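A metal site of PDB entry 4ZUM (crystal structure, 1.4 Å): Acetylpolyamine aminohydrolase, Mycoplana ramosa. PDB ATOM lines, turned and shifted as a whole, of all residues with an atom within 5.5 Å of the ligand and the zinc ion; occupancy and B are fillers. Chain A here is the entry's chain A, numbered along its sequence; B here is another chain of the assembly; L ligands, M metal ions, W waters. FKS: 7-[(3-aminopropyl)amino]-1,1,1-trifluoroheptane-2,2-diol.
OE2 of Glu 106 of chain B lies within salt-bridge range of N1 of the ligand (2.8 Å). O14 of the ligand sits close to NE2 of His 158 (2.7 Å). OH of Tyr 83 of chain B is in hydrogen-bond range of N1 of the ligand (3.4 Å). An oxygen (O13) of the ligand sits close to the side-chain hydroxyl (OH) of Tyr 323 (2.6 Å). O14 of the ligand sits close to NE2 of His 159, at 2.7 Å.
OE2 of Glu 17 sits at hydrogen-bond distance from OH of Tyr 168, 2.6 Å away. SG of Cys 169 sits at hydrogen-bond distance from N of His 158. OD1 of Asp 284 sits at hydrogen-bond distance from N of Phe 196 (2.8 Å). The side-chain sulfur (SG) of Cys 169 lies within hydrogen-bond range of the backbone NH (N) of Gly 157 (3.4 Å). The side-chain carboxylate (OE1) of Glu 320 lies within hydrogen-bond range of the backbone NH (N) of Gly 157 (3.0 Å). NE2 of His 159 lies within hydrogen-bond range of NE2 of His 158, 3.3 Å away. The backbone NH (N) of Gly 167 lies within hydrogen-bond range of the side-chain carboxylate (OE2) of Glu 117. N of His 158 sits at hydrogen-bond distance from OE1 of Glu 320 (3.0 Å).
A fluorine (F15) of the ligand sits close to the backbone carbonyl oxygen (O) of Gly 167, at 3.3 Å. A fluorine (F15) of the ligand sits close to the side-chain sulfur (SG) of Cys 169. A fluorine (F16) of the ligand sits close to the backbone NH (N) of Gly 321 (3.0 Å). Pro 156 touches the ligand (CG to F17, 3.2 Å). CD2 of Tyr 168 touches C10 of the ligand (3.6 Å). Phe 225 touches the ligand. Ile 291 touches the ligand (CD1 to C7, 3.9 Å). Glu 320 touches the ligand (CB to F16, 3.4 Å). Hydrophobic or aromatic side chains within 4 Å of the ligand: Pro 156, His 158, His 159, Tyr 168, His 197, Phe 225, Ile 291 and Tyr 323.
The nearest printed residue that does not touch the zinc ion is Phe 196 (4.3 Å).
The zinc ion is bound by the side-chain carboxylate (OD2) of Asp 284 (2.0 Å), the side-chain carboxylate (OD1) of Asp 195 (2.0 Å), an oxygen (O13) of the ligand (2.0 Å), a ring nitrogen (ND1) of His 197 (2.1 Å) and an oxygen (O14) of the ligand (2.4 Å). Slightly farther from the zinc ion lies the side-chain carboxylate (OD2) of Asp 195 (2.8 Å).
Water W3 lies within hydrogen-bond range of OE2 of Glu 17 (2.5 Å) and N5 of the ligand (2.8 Å). Water W2 bridges OE1 of Glu 117 (2.7 Å) and N5 of the ligand (2.9 Å). Water W1 bridges O of Ile 291 (2.7 Å) and NE2 of His 197 (2.8 Å).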
ATOM      1  N   GLU A  17     -11.773   5.862 -18.551  1.00  0.00           N
ATOM      2  CA  GLU A  17     -12.731   5.093 -17.788  1.00  0.00           C
ATOM      3  C   GLU A  17     -12.699   3.668 -18.322  1.00  0.00           C
ATOM      4  O   GLU A  17     -12.704   3.462 -19.533  1.00  0.00           O
ATOM      5  CB  GLU A  17     -14.150   5.678 -17.960  1.00  0.00           C
ATOM      6  CG  GLU A  17     -15.250   4.796 -17.364  1.00  0.00           C
ATOM      7  CD  GLU A  17     -16.621   5.441 -17.390  1.00  0.00           C
ATOM      8  OE1 GLU A  17     -16.732   6.677 -17.609  1.00  0.00           O
ATOM      9  OE2 GLU A  17     -17.580   4.682 -17.152  1.00  0.00           O
ATOM     10  N   TYR A  19     -14.459   0.671 -19.356  1.00  0.00           N
ATOM     11  CA  TYR A  19     -15.832   0.334 -19.755  1.00  0.00           C
ATOM     12  C   TYR A  19     -15.778  -0.714 -20.876  1.00  0.00           C
ATOM     13  O   TYR A  19     -15.126  -0.507 -21.907  1.00  0.00           O
ATOM     14  CB  TYR A  19     -16.550   1.600 -20.248  1.00  0.00           C
ATOM     15  CG  TYR A  19     -17.926   1.323 -20.802  1.00  0.00           C
ATOM     16  CD1 TYR A  19     -18.975   1.004 -19.947  1.00  0.00           C
ATOM     17  CD2 TYR A  19     -18.170   1.382 -22.149  1.00  0.00           C
ATOM     18  CE1 TYR A  19     -20.230   0.740 -20.431  1.00  0.00           C
ATOM     19  CE2 TYR A  19     -19.432   1.122 -22.645  1.00  0.00           C
ATOM     20  CZ  TYR A  19     -20.452   0.809 -21.781  1.00  0.00           C
ATOM     21  OH  TYR A  19     -21.714   0.539 -22.280  1.00  0.00           O
ATOM     22  N   GLU A  28     -18.571  10.723 -17.177  1.00  0.00           N
ATOM     23  CA  GLU A  28     -18.747  11.798 -16.198  1.00  0.00           C
ATOM     24  C   GLU A  28     -17.720  12.902 -16.475  1.00  0.00           C
ATOM     25  O   GLU A  28     -16.683  13.029 -15.812  1.00  0.00           O
ATOM     26  CB  GLU A  28     -18.659  11.222 -14.778  1.00  0.00           C
ATOM     27  CG  GLU A  28     -19.340  12.086 -13.711  1.00  0.00           C
ATOM     28  CD  GLU A  28     -18.791  13.494 -13.652  1.00  0.00           C
ATOM     29  OE1 GLU A  28     -17.849  13.754 -12.853  1.00  0.00           O
ATOM     30  OE2 GLU A  28     -19.282  14.345 -14.422  1.00  0.00           O
ATOM     31  N   GLU A 117     -14.029   1.179 -12.568  1.00  0.00           N
ATOM     32  CA  GLU A 117     -14.191   1.997 -13.750  1.00  0.00           C
ATOM     33  C   GLU A 117     -13.722   3.433 -13.536  1.00  0.00           C
ATOM     34  O   GLU A 117     -13.436   4.136 -14.516  1.00  0.00           O
ATOM     35  CB  GLU A 117     -15.625   1.997 -14.267  1.00  0.00           C
ATOM     36  CG  GLU A 117     -16.572   2.909 -13.524  1.00  0.00           C
ATOM     37  CD  GLU A 117     -16.869   2.386 -12.149  1.00  0.00           C
ATOM     38  OE1 GLU A 117     -17.165   1.181 -12.033  1.00  0.00           O
ATOM     39  OE2 GLU A 117     -16.727   3.155 -11.183  1.00  0.00           O
ATOM     40  N   PRO A 156     -20.032  13.791  -8.864  1.00  0.00           N
ATOM     41  CA  PRO A 156     -21.173  13.333  -8.085  1.00  0.00           C
ATOM     42  C   PRO A 156     -20.708  12.580  -6.846  1.00  0.00           C
ATOM     43  O   PRO A 156     -19.495  12.391  -6.654  1.00  0.00           O
ATOM     44  CB  PRO A 156     -21.899  12.392  -9.055  1.00  0.00           C
ATOM     45  CG  PRO A 156     -20.767  11.817  -9.910  1.00  0.00           C
ATOM     46  CD  PRO A 156     -19.850  13.011 -10.103  1.00  0.00           C
ATOM     47  N   GLY A 157     -21.659  12.136  -6.035  1.00  0.00           N
ATOM     48  CA  GLY A 157     -21.316  11.651  -4.703  1.00  0.00           C
ATOM     49  C   GLY A 157     -21.895  10.337  -4.228  1.00  0.00           C
ATOM     50  O   GLY A 157     -21.278   9.724  -3.337  1.00  0.00           O
ATOM     51  N   HIS A 158     -23.018   9.855  -4.773  1.00  0.00           N
ATOM     52  CA  HIS A 158     -23.787   8.863  -4.003  1.00  0.00           C
ATOM     53  C   HIS A 158     -23.233   7.433  -3.988  1.00  0.00           C
ATOM     54  O   HIS A 158     -23.711   6.622  -3.185  1.00  0.00           O
ATOM     55  CB  HIS A 158     -25.270   8.864  -4.379  1.00  0.00           C
ATOM     56  CG  HIS A 158     -25.564   8.304  -5.733  1.00  0.00           C
ATOM     57  ND1 HIS A 158     -26.804   7.767  -6.042  1.00  0.00           N
ATOM     58  CD2 HIS A 158     -24.807   8.186  -6.849  1.00  0.00           C
ATOM     59  CE1 HIS A 158     -26.793   7.342  -7.300  1.00  0.00           C
ATOM     60  NE2 HIS A 158     -25.591   7.575  -7.808  1.00  0.00           N
ATOM     61  N   HIS A 159     -22.222   7.136  -4.800  1.00  0.00           N
ATOM     62  CA  HIS A 159     -21.526   5.843  -4.708  1.00  0.00           C
ATOM     63  C   HIS A 159     -20.380   5.826  -3.709  1.00  0.00           C
ATOM     64  O   HIS A 159     -19.825   4.756  -3.458  1.00  0.00           O
ATOM     65  CB  HIS A 159     -21.029   5.346  -6.068  1.00  0.00           C
ATOM     66  CG  HIS A 159     -22.118   5.152  -7.055  1.00  0.00           C
ATOM     67  ND1 HIS A 159     -23.166   4.271  -6.853  1.00  0.00           N
ATOM     68  CD2 HIS A 159     -22.333   5.735  -8.262  1.00  0.00           C
ATOM     69  CE1 HIS A 159     -23.989   4.337  -7.894  1.00  0.00           C
ATOM     70  NE2 HIS A 159     -23.499   5.208  -8.770  1.00  0.00           N
ATOM     71  N   GLY A 167     -17.810   4.493  -8.927  1.00  0.00           N
ATOM     72  CA  GLY A 167     -18.981   5.009  -9.633  1.00  0.00           C
ATOM     73  C   GLY A 167     -18.897   6.515  -9.898  1.00  0.00           C
ATOM     74  O   GLY A 167     -19.914   7.222  -9.810  1.00  0.00           O
ATOM     75  N   TYR A 168     -17.685   6.998 -10.166  1.00  0.00           N
ATOM     76  CA  TYR A 168     -17.436   8.400 -10.537  1.00  0.00           C
ATOM     77  C   TYR A 168     -17.469   9.349  -9.328  1.00  0.00           C
ATOM     78  O   TYR A 168     -17.388  10.569  -9.493  1.00  0.00           O
ATOM     79  CB  TYR A 168     -18.440   8.928 -11.592  1.00  0.00           C
ATOM     80  CG  TYR A 168     -18.766   8.034 -12.773  1.00  0.00           C
ATOM     81  CD1 TYR A 168     -17.907   7.024 -13.202  1.00  0.00           C
ATOM     82  CD2 TYR A 168     -19.947   8.246 -13.498  1.00  0.00           C
ATOM     83  CE1 TYR A 168     -18.220   6.226 -14.299  1.00  0.00           C
ATOM     84  CE2 TYR A 168     -20.264   7.484 -14.604  1.00  0.00           C
ATOM     85  CZ  TYR A 168     -19.402   6.472 -15.000  1.00  0.00           C
ATOM     86  OH  TYR A 168     -19.737   5.730 -16.103  1.00  0.00           O
ATOM     87  N   CYS A 169     -17.534   8.781  -8.109  1.00  0.00           N
ATOM     88  CA  CYS A 169     -17.799   9.527  -6.882  1.00  0.00           C
ATOM     89  C   CYS A 169     -16.658   9.374  -5.892  1.00  0.00           C
ATOM     90  O   CYS A 169     -16.091   8.292  -5.752  1.00  0.00           O
ATOM     91  CB  CYS A 169     -19.038   8.956  -6.193  1.00  0.00           C
ATOM     92  SG  CYS A 169     -20.566   9.084  -7.169  1.00  0.00           S
ATOM     93  N   ASP A 195     -31.606   9.210  -8.779  1.00  0.00           N
ATOM     94  CA  ASP A 195     -30.676   8.778  -9.818  1.00  0.00           C
ATOM     95  C   ASP A 195     -31.007   7.337 -10.196  1.00  0.00           C
ATOM     96  O   ASP A 195     -31.505   6.571  -9.371  1.00  0.00           O
ATOM     97  CB  ASP A 195     -29.249   8.933  -9.232  1.00  0.00           C
ATOM     98  CG  ASP A 195     -28.147   8.650 -10.225  1.00  0.00           C
ATOM     99  OD1 ASP A 195     -27.876   7.459 -10.499  1.00  0.00           O
ATOM    100  OD2 ASP A 195     -27.536   9.606 -10.751  1.00  0.00           O
ATOM    101  N   PHE A 196     -30.763   6.971 -11.460  1.00  0.00           N
ATOM    102  CA  PHE A 196     -31.033   5.594 -11.898  1.00  0.00           C
ATOM    103  C   PHE A 196     -30.316   4.558 -11.032  1.00  0.00           C
ATOM    104  O   PHE A 196     -30.831   3.461 -10.842  1.00  0.00           O
ATOM    105  CB  PHE A 196     -30.604   5.423 -13.349  1.00  0.00           C
ATOM    106  CG  PHE A 196     -30.626   4.006 -13.815  1.00  0.00           C
ATOM    107  CD1 PHE A 196     -31.837   3.395 -14.157  1.00  0.00           C
ATOM    108  CD2 PHE A 196     -29.452   3.266 -13.886  1.00  0.00           C
ATOM    109  CE1 PHE A 196     -31.854   2.059 -14.558  1.00  0.00           C
ATOM    110  CE2 PHE A 196     -29.468   1.930 -14.287  1.00  0.00           C
ATOM    111  CZ  PHE A 196     -30.670   1.327 -14.623  1.00  0.00           C
ATOM    112  N   HIS A 197     -29.110   4.862 -10.588  1.00  0.00           N
ATOM    113  CA  HIS A 197     -28.306   3.904  -9.846  1.00  0.00           C
ATOM    114  C   HIS A 197     -28.572   3.966  -8.351  1.00  0.00           C
ATOM    115  O   HIS A 197     -28.884   5.041  -7.803  1.00  0.00           O
ATOM    116  CB  HIS A 197     -26.811   4.155 -10.120  1.00  0.00           C
ATOM    117  CG  HIS A 197     -26.471   4.105 -11.569  1.00  0.00           C
ATOM    118  ND1 HIS A 197     -26.447   5.227 -12.390  1.00  0.00           N
ATOM    119  CD2 HIS A 197     -26.167   3.051 -12.365  1.00  0.00           C
ATOM    120  CE1 HIS A 197     -26.159   4.840 -13.629  1.00  0.00           C
ATOM    121  NE2 HIS A 197     -25.989   3.527 -13.634  1.00  0.00           N
ATOM    122  N   PHE A 225     -25.532  -1.727 -12.160  1.00  0.00           N
ATOM    123  CA  PHE A 225     -24.535  -1.129 -11.295  1.00  0.00           C
ATOM    124  C   PHE A 225     -25.298  -0.365 -10.187  1.00  0.00           C
ATOM    125  O   PHE A 225     -26.299   0.293 -10.444  1.00  0.00           O
ATOM    126  CB  PHE A 225     -23.711  -0.127 -12.124  1.00  0.00           C
ATOM    127  CG  PHE A 225     -22.595   0.510 -11.368  1.00  0.00           C
ATOM    128  CD1 PHE A 225     -21.341  -0.045 -11.370  1.00  0.00           C
ATOM    129  CD2 PHE A 225     -22.806   1.646 -10.627  1.00  0.00           C
ATOM    130  CE1 PHE A 225     -20.286   0.514 -10.659  1.00  0.00           C
ATOM    131  CE2 PHE A 225     -21.783   2.229  -9.894  1.00  0.00           C
ATOM    132  CZ  PHE A 225     -20.511   1.644  -9.903  1.00  0.00           C
ATOM    133  N   ASP A 284     -30.223  10.224 -15.189  1.00  0.00           N
ATOM    134  CA  ASP A 284     -29.925   9.041 -15.981  1.00  0.00           C
ATOM    135  C   ASP A 284     -31.076   8.038 -16.038  1.00  0.00           C
ATOM    136  O   ASP A 284     -30.940   6.998 -16.662  1.00  0.00           O
ATOM    137  CB  ASP A 284     -28.602   8.350 -15.555  1.00  0.00           C
ATOM    138  CG  ASP A 284     -28.402   8.250 -14.070  1.00  0.00           C
ATOM    139  OD1 ASP A 284     -29.293   8.589 -13.265  1.00  0.00           O
ATOM    140  OD2 ASP A 284     -27.276   7.802 -13.701  1.00  0.00           O
ATOM    141  N   ILE A 291     -26.260   4.678 -20.422  1.00  0.00           N
ATOM    142  CA  ILE A 291     -25.838   3.577 -19.557  1.00  0.00           C
ATOM    143  C   ILE A 291     -26.953   2.993 -18.677  1.00  0.00           C
ATOM    144  O   ILE A 291     -26.682   2.179 -17.818  1.00  0.00           O
ATOM    145  CB  ILE A 291     -24.592   3.963 -18.720  1.00  0.00           C
ATOM    146  CG1 ILE A 291     -24.894   5.105 -17.737  1.00  0.00           C
ATOM    147  CG2 ILE A 291     -23.403   4.294 -19.645  1.00  0.00           C
ATOM    148  CD1 ILE A 291     -23.710   5.308 -16.755  1.00  0.00           C
ATOM    149  N   GLU A 320     -26.380  14.535  -9.225  1.00  0.00           N
ATOM    150  CA  GLU A 320     -25.702  13.237  -9.337  1.00  0.00           C
ATOM    151  C   GLU A 320     -25.424  12.943 -10.818  1.00  0.00           C
ATOM    152  O   GLU A 320     -24.726  13.720 -11.467  1.00  0.00           O
ATOM    153  CB  GLU A 320     -26.504  12.117  -8.624  1.00  0.00           C
ATOM    154  CG  GLU A 320     -26.787  12.413  -7.121  1.00  0.00           C
ATOM    155  CD  GLU A 320     -25.622  12.122  -6.167  1.00  0.00           C
ATOM    156  OE1 GLU A 320     -24.534  11.675  -6.599  1.00  0.00           O
ATOM    157  OE2 GLU A 320     -25.816  12.329  -4.939  1.00  0.00           O
ATOM    158  N   GLY A 321     -25.996  11.868 -11.371  1.00  0.00           N
ATOM    159  CA  GLY A 321     -25.685  11.444 -12.739  1.00  0.00           C
ATOM    160  C   GLY A 321     -26.648  11.915 -13.816  1.00  0.00           C
ATOM    161  O   GLY A 321     -27.469  12.807 -13.587  1.00  0.00           O
ATOM    162  N   GLY A 322     -26.529  11.319 -15.002  1.00  0.00           N
ATOM    163  CA  GLY A 322     -27.217  11.763 -16.228  1.00  0.00           C
ATOM    164  C   GLY A 322     -26.168  12.083 -17.280  1.00  0.00           C
ATOM    165  O   GLY A 322     -25.329  12.963 -17.074  1.00  0.00           O
ATOM    166  N   TYR A 323     -26.224  11.388 -18.416  1.00  0.00           N
ATOM    167  CA  TYR A 323     -25.089  11.308 -19.356  1.00  0.00           C
ATOM    168  C   TYR A 323     -25.456  11.523 -20.819  1.00  0.00           C
ATOM    169  O   TYR A 323     -26.627  11.454 -21.208  1.00  0.00           O
ATOM    170  CB  TYR A 323     -24.411   9.926 -19.225  1.00  0.00           C
ATOM    171  CG  TYR A 323     -24.016   9.714 -17.798  1.00  0.00           C
ATOM    172  CD1 TYR A 323     -24.801   8.950 -16.924  1.00  0.00           C
ATOM    173  CD2 TYR A 323     -22.908  10.386 -17.273  1.00  0.00           C
ATOM    174  CE1 TYR A 323     -24.471   8.835 -15.576  1.00  0.00           C
ATOM    175  CE2 TYR A 323     -22.566  10.273 -15.932  1.00  0.00           C
ATOM    176  CZ  TYR A 323     -23.354   9.502 -15.095  1.00  0.00           C
ATOM    177  OH  TYR A 323     -23.029   9.404 -13.763  1.00  0.00           O
ATOM    178  N   TYR B  83     -20.029  -5.964 -25.464  1.00  0.00           N
ATOM    179  CA  TYR B  83     -18.781  -5.308 -25.075  1.00  0.00           C
ATOM    180  C   TYR B  83     -17.684  -5.556 -26.078  1.00  0.00           C
ATOM    181  O   TYR B  83     -17.613  -6.617 -26.694  1.00  0.00           O
ATOM    182  CB  TYR B  83     -18.375  -5.736 -23.672  1.00  0.00           C
ATOM    183  CG  TYR B  83     -19.377  -5.270 -22.661  1.00  0.00           C
ATOM    184  CD1 TYR B  83     -19.677  -3.917 -22.554  1.00  0.00           C
ATOM    185  CD2 TYR B  83     -20.051  -6.172 -21.855  1.00  0.00           C
ATOM    186  CE1 TYR B  83     -20.608  -3.474 -21.654  1.00  0.00           C
ATOM    187  CE2 TYR B  83     -20.993  -5.731 -20.949  1.00  0.00           C
ATOM    188  CZ  TYR B  83     -21.262  -4.388 -20.848  1.00  0.00           C
ATOM    189  OH  TYR B  83     -22.195  -3.957 -19.943  1.00  0.00           O
ATOM    190  N   GLU B 106     -22.054  -8.427 -16.151  1.00  0.00           N
ATOM    191  CA  GLU B 106     -21.180  -7.452 -15.472  1.00  0.00           C
ATOM    192  C   GLU B 106     -21.206  -7.683 -13.961  1.00  0.00           C
ATOM    193  O   GLU B 106     -20.161  -7.742 -13.289  1.00  0.00           O
ATOM    194  CB  GLU B 106     -21.580  -6.007 -15.816  1.00  0.00           C
ATOM    195  CG  GLU B 106     -20.857  -4.929 -15.003  1.00  0.00           C
ATOM    196  CD  GLU B 106     -21.256  -3.532 -15.475  1.00  0.00           C
ATOM    197  OE1 GLU B 106     -22.009  -2.827 -14.739  1.00  0.00           O
ATOM    198  OE2 GLU B 106     -20.825  -3.157 -16.587  1.00  0.00           O
HETATM  199  C2  FKS L   1     -22.827  -0.435 -16.688  1.00  0.00           C
HETATM  200  C3  FKS L   1     -21.594   0.387 -16.338  1.00  0.00           C
HETATM  201  C4  FKS L   1     -21.825   1.260 -15.109  1.00  0.00           C
HETATM  202  C6  FKS L   1     -20.642   2.961 -13.647  1.00  0.00           C
HETATM  203  C7  FKS L   1     -21.856   3.902 -13.674  1.00  0.00           C
HETATM  204  C8  FKS L   1     -21.729   4.888 -12.520  1.00  0.00           C
HETATM  205  C9  FKS L   1     -22.985   5.769 -12.472  1.00  0.00           C
HETATM  206  C10 FKS L   1     -22.716   7.005 -11.615  1.00  0.00           C
HETATM  207  C11 FKS L   1     -23.964   7.762 -11.139  1.00  0.00           C
HETATM  208  C12 FKS L   1     -23.579   8.997 -10.342  1.00  0.00           C
HETATM  209  F15 FKS L   1     -22.785   8.710  -9.337  1.00  0.00           F
HETATM  210  F16 FKS L   1     -24.705   9.566  -9.862  1.00  0.00           F
HETATM  211  F17 FKS L   1     -22.982   9.887 -11.083  1.00  0.00           F
HETATM  212  N5  FKS L   1     -20.632   2.039 -14.785  1.00  0.00           N
HETATM  213  N1  FKS L   1     -22.514  -1.295 -17.815  1.00  0.00           N
HETATM  214  O13 FKS L   1     -24.755   8.163 -12.243  1.00  0.00           O
HETATM  215  O14 FKS L   1     -24.799   6.948 -10.297  1.00  0.00           O
HETATM  216 ZN    ZN M   1     -26.530   7.247 -11.974  1.00  0.00          ZN
HETATM  217  O   HOH W   1     -25.158   1.757 -15.612  1.00  0.00           O
HETATM  218  O   HOH W   2     -18.607   0.093 -13.977  1.00  0.00           O
HETATM  219  O   HOH W   3     -18.616   2.391 -16.746  1.00  0.00           O
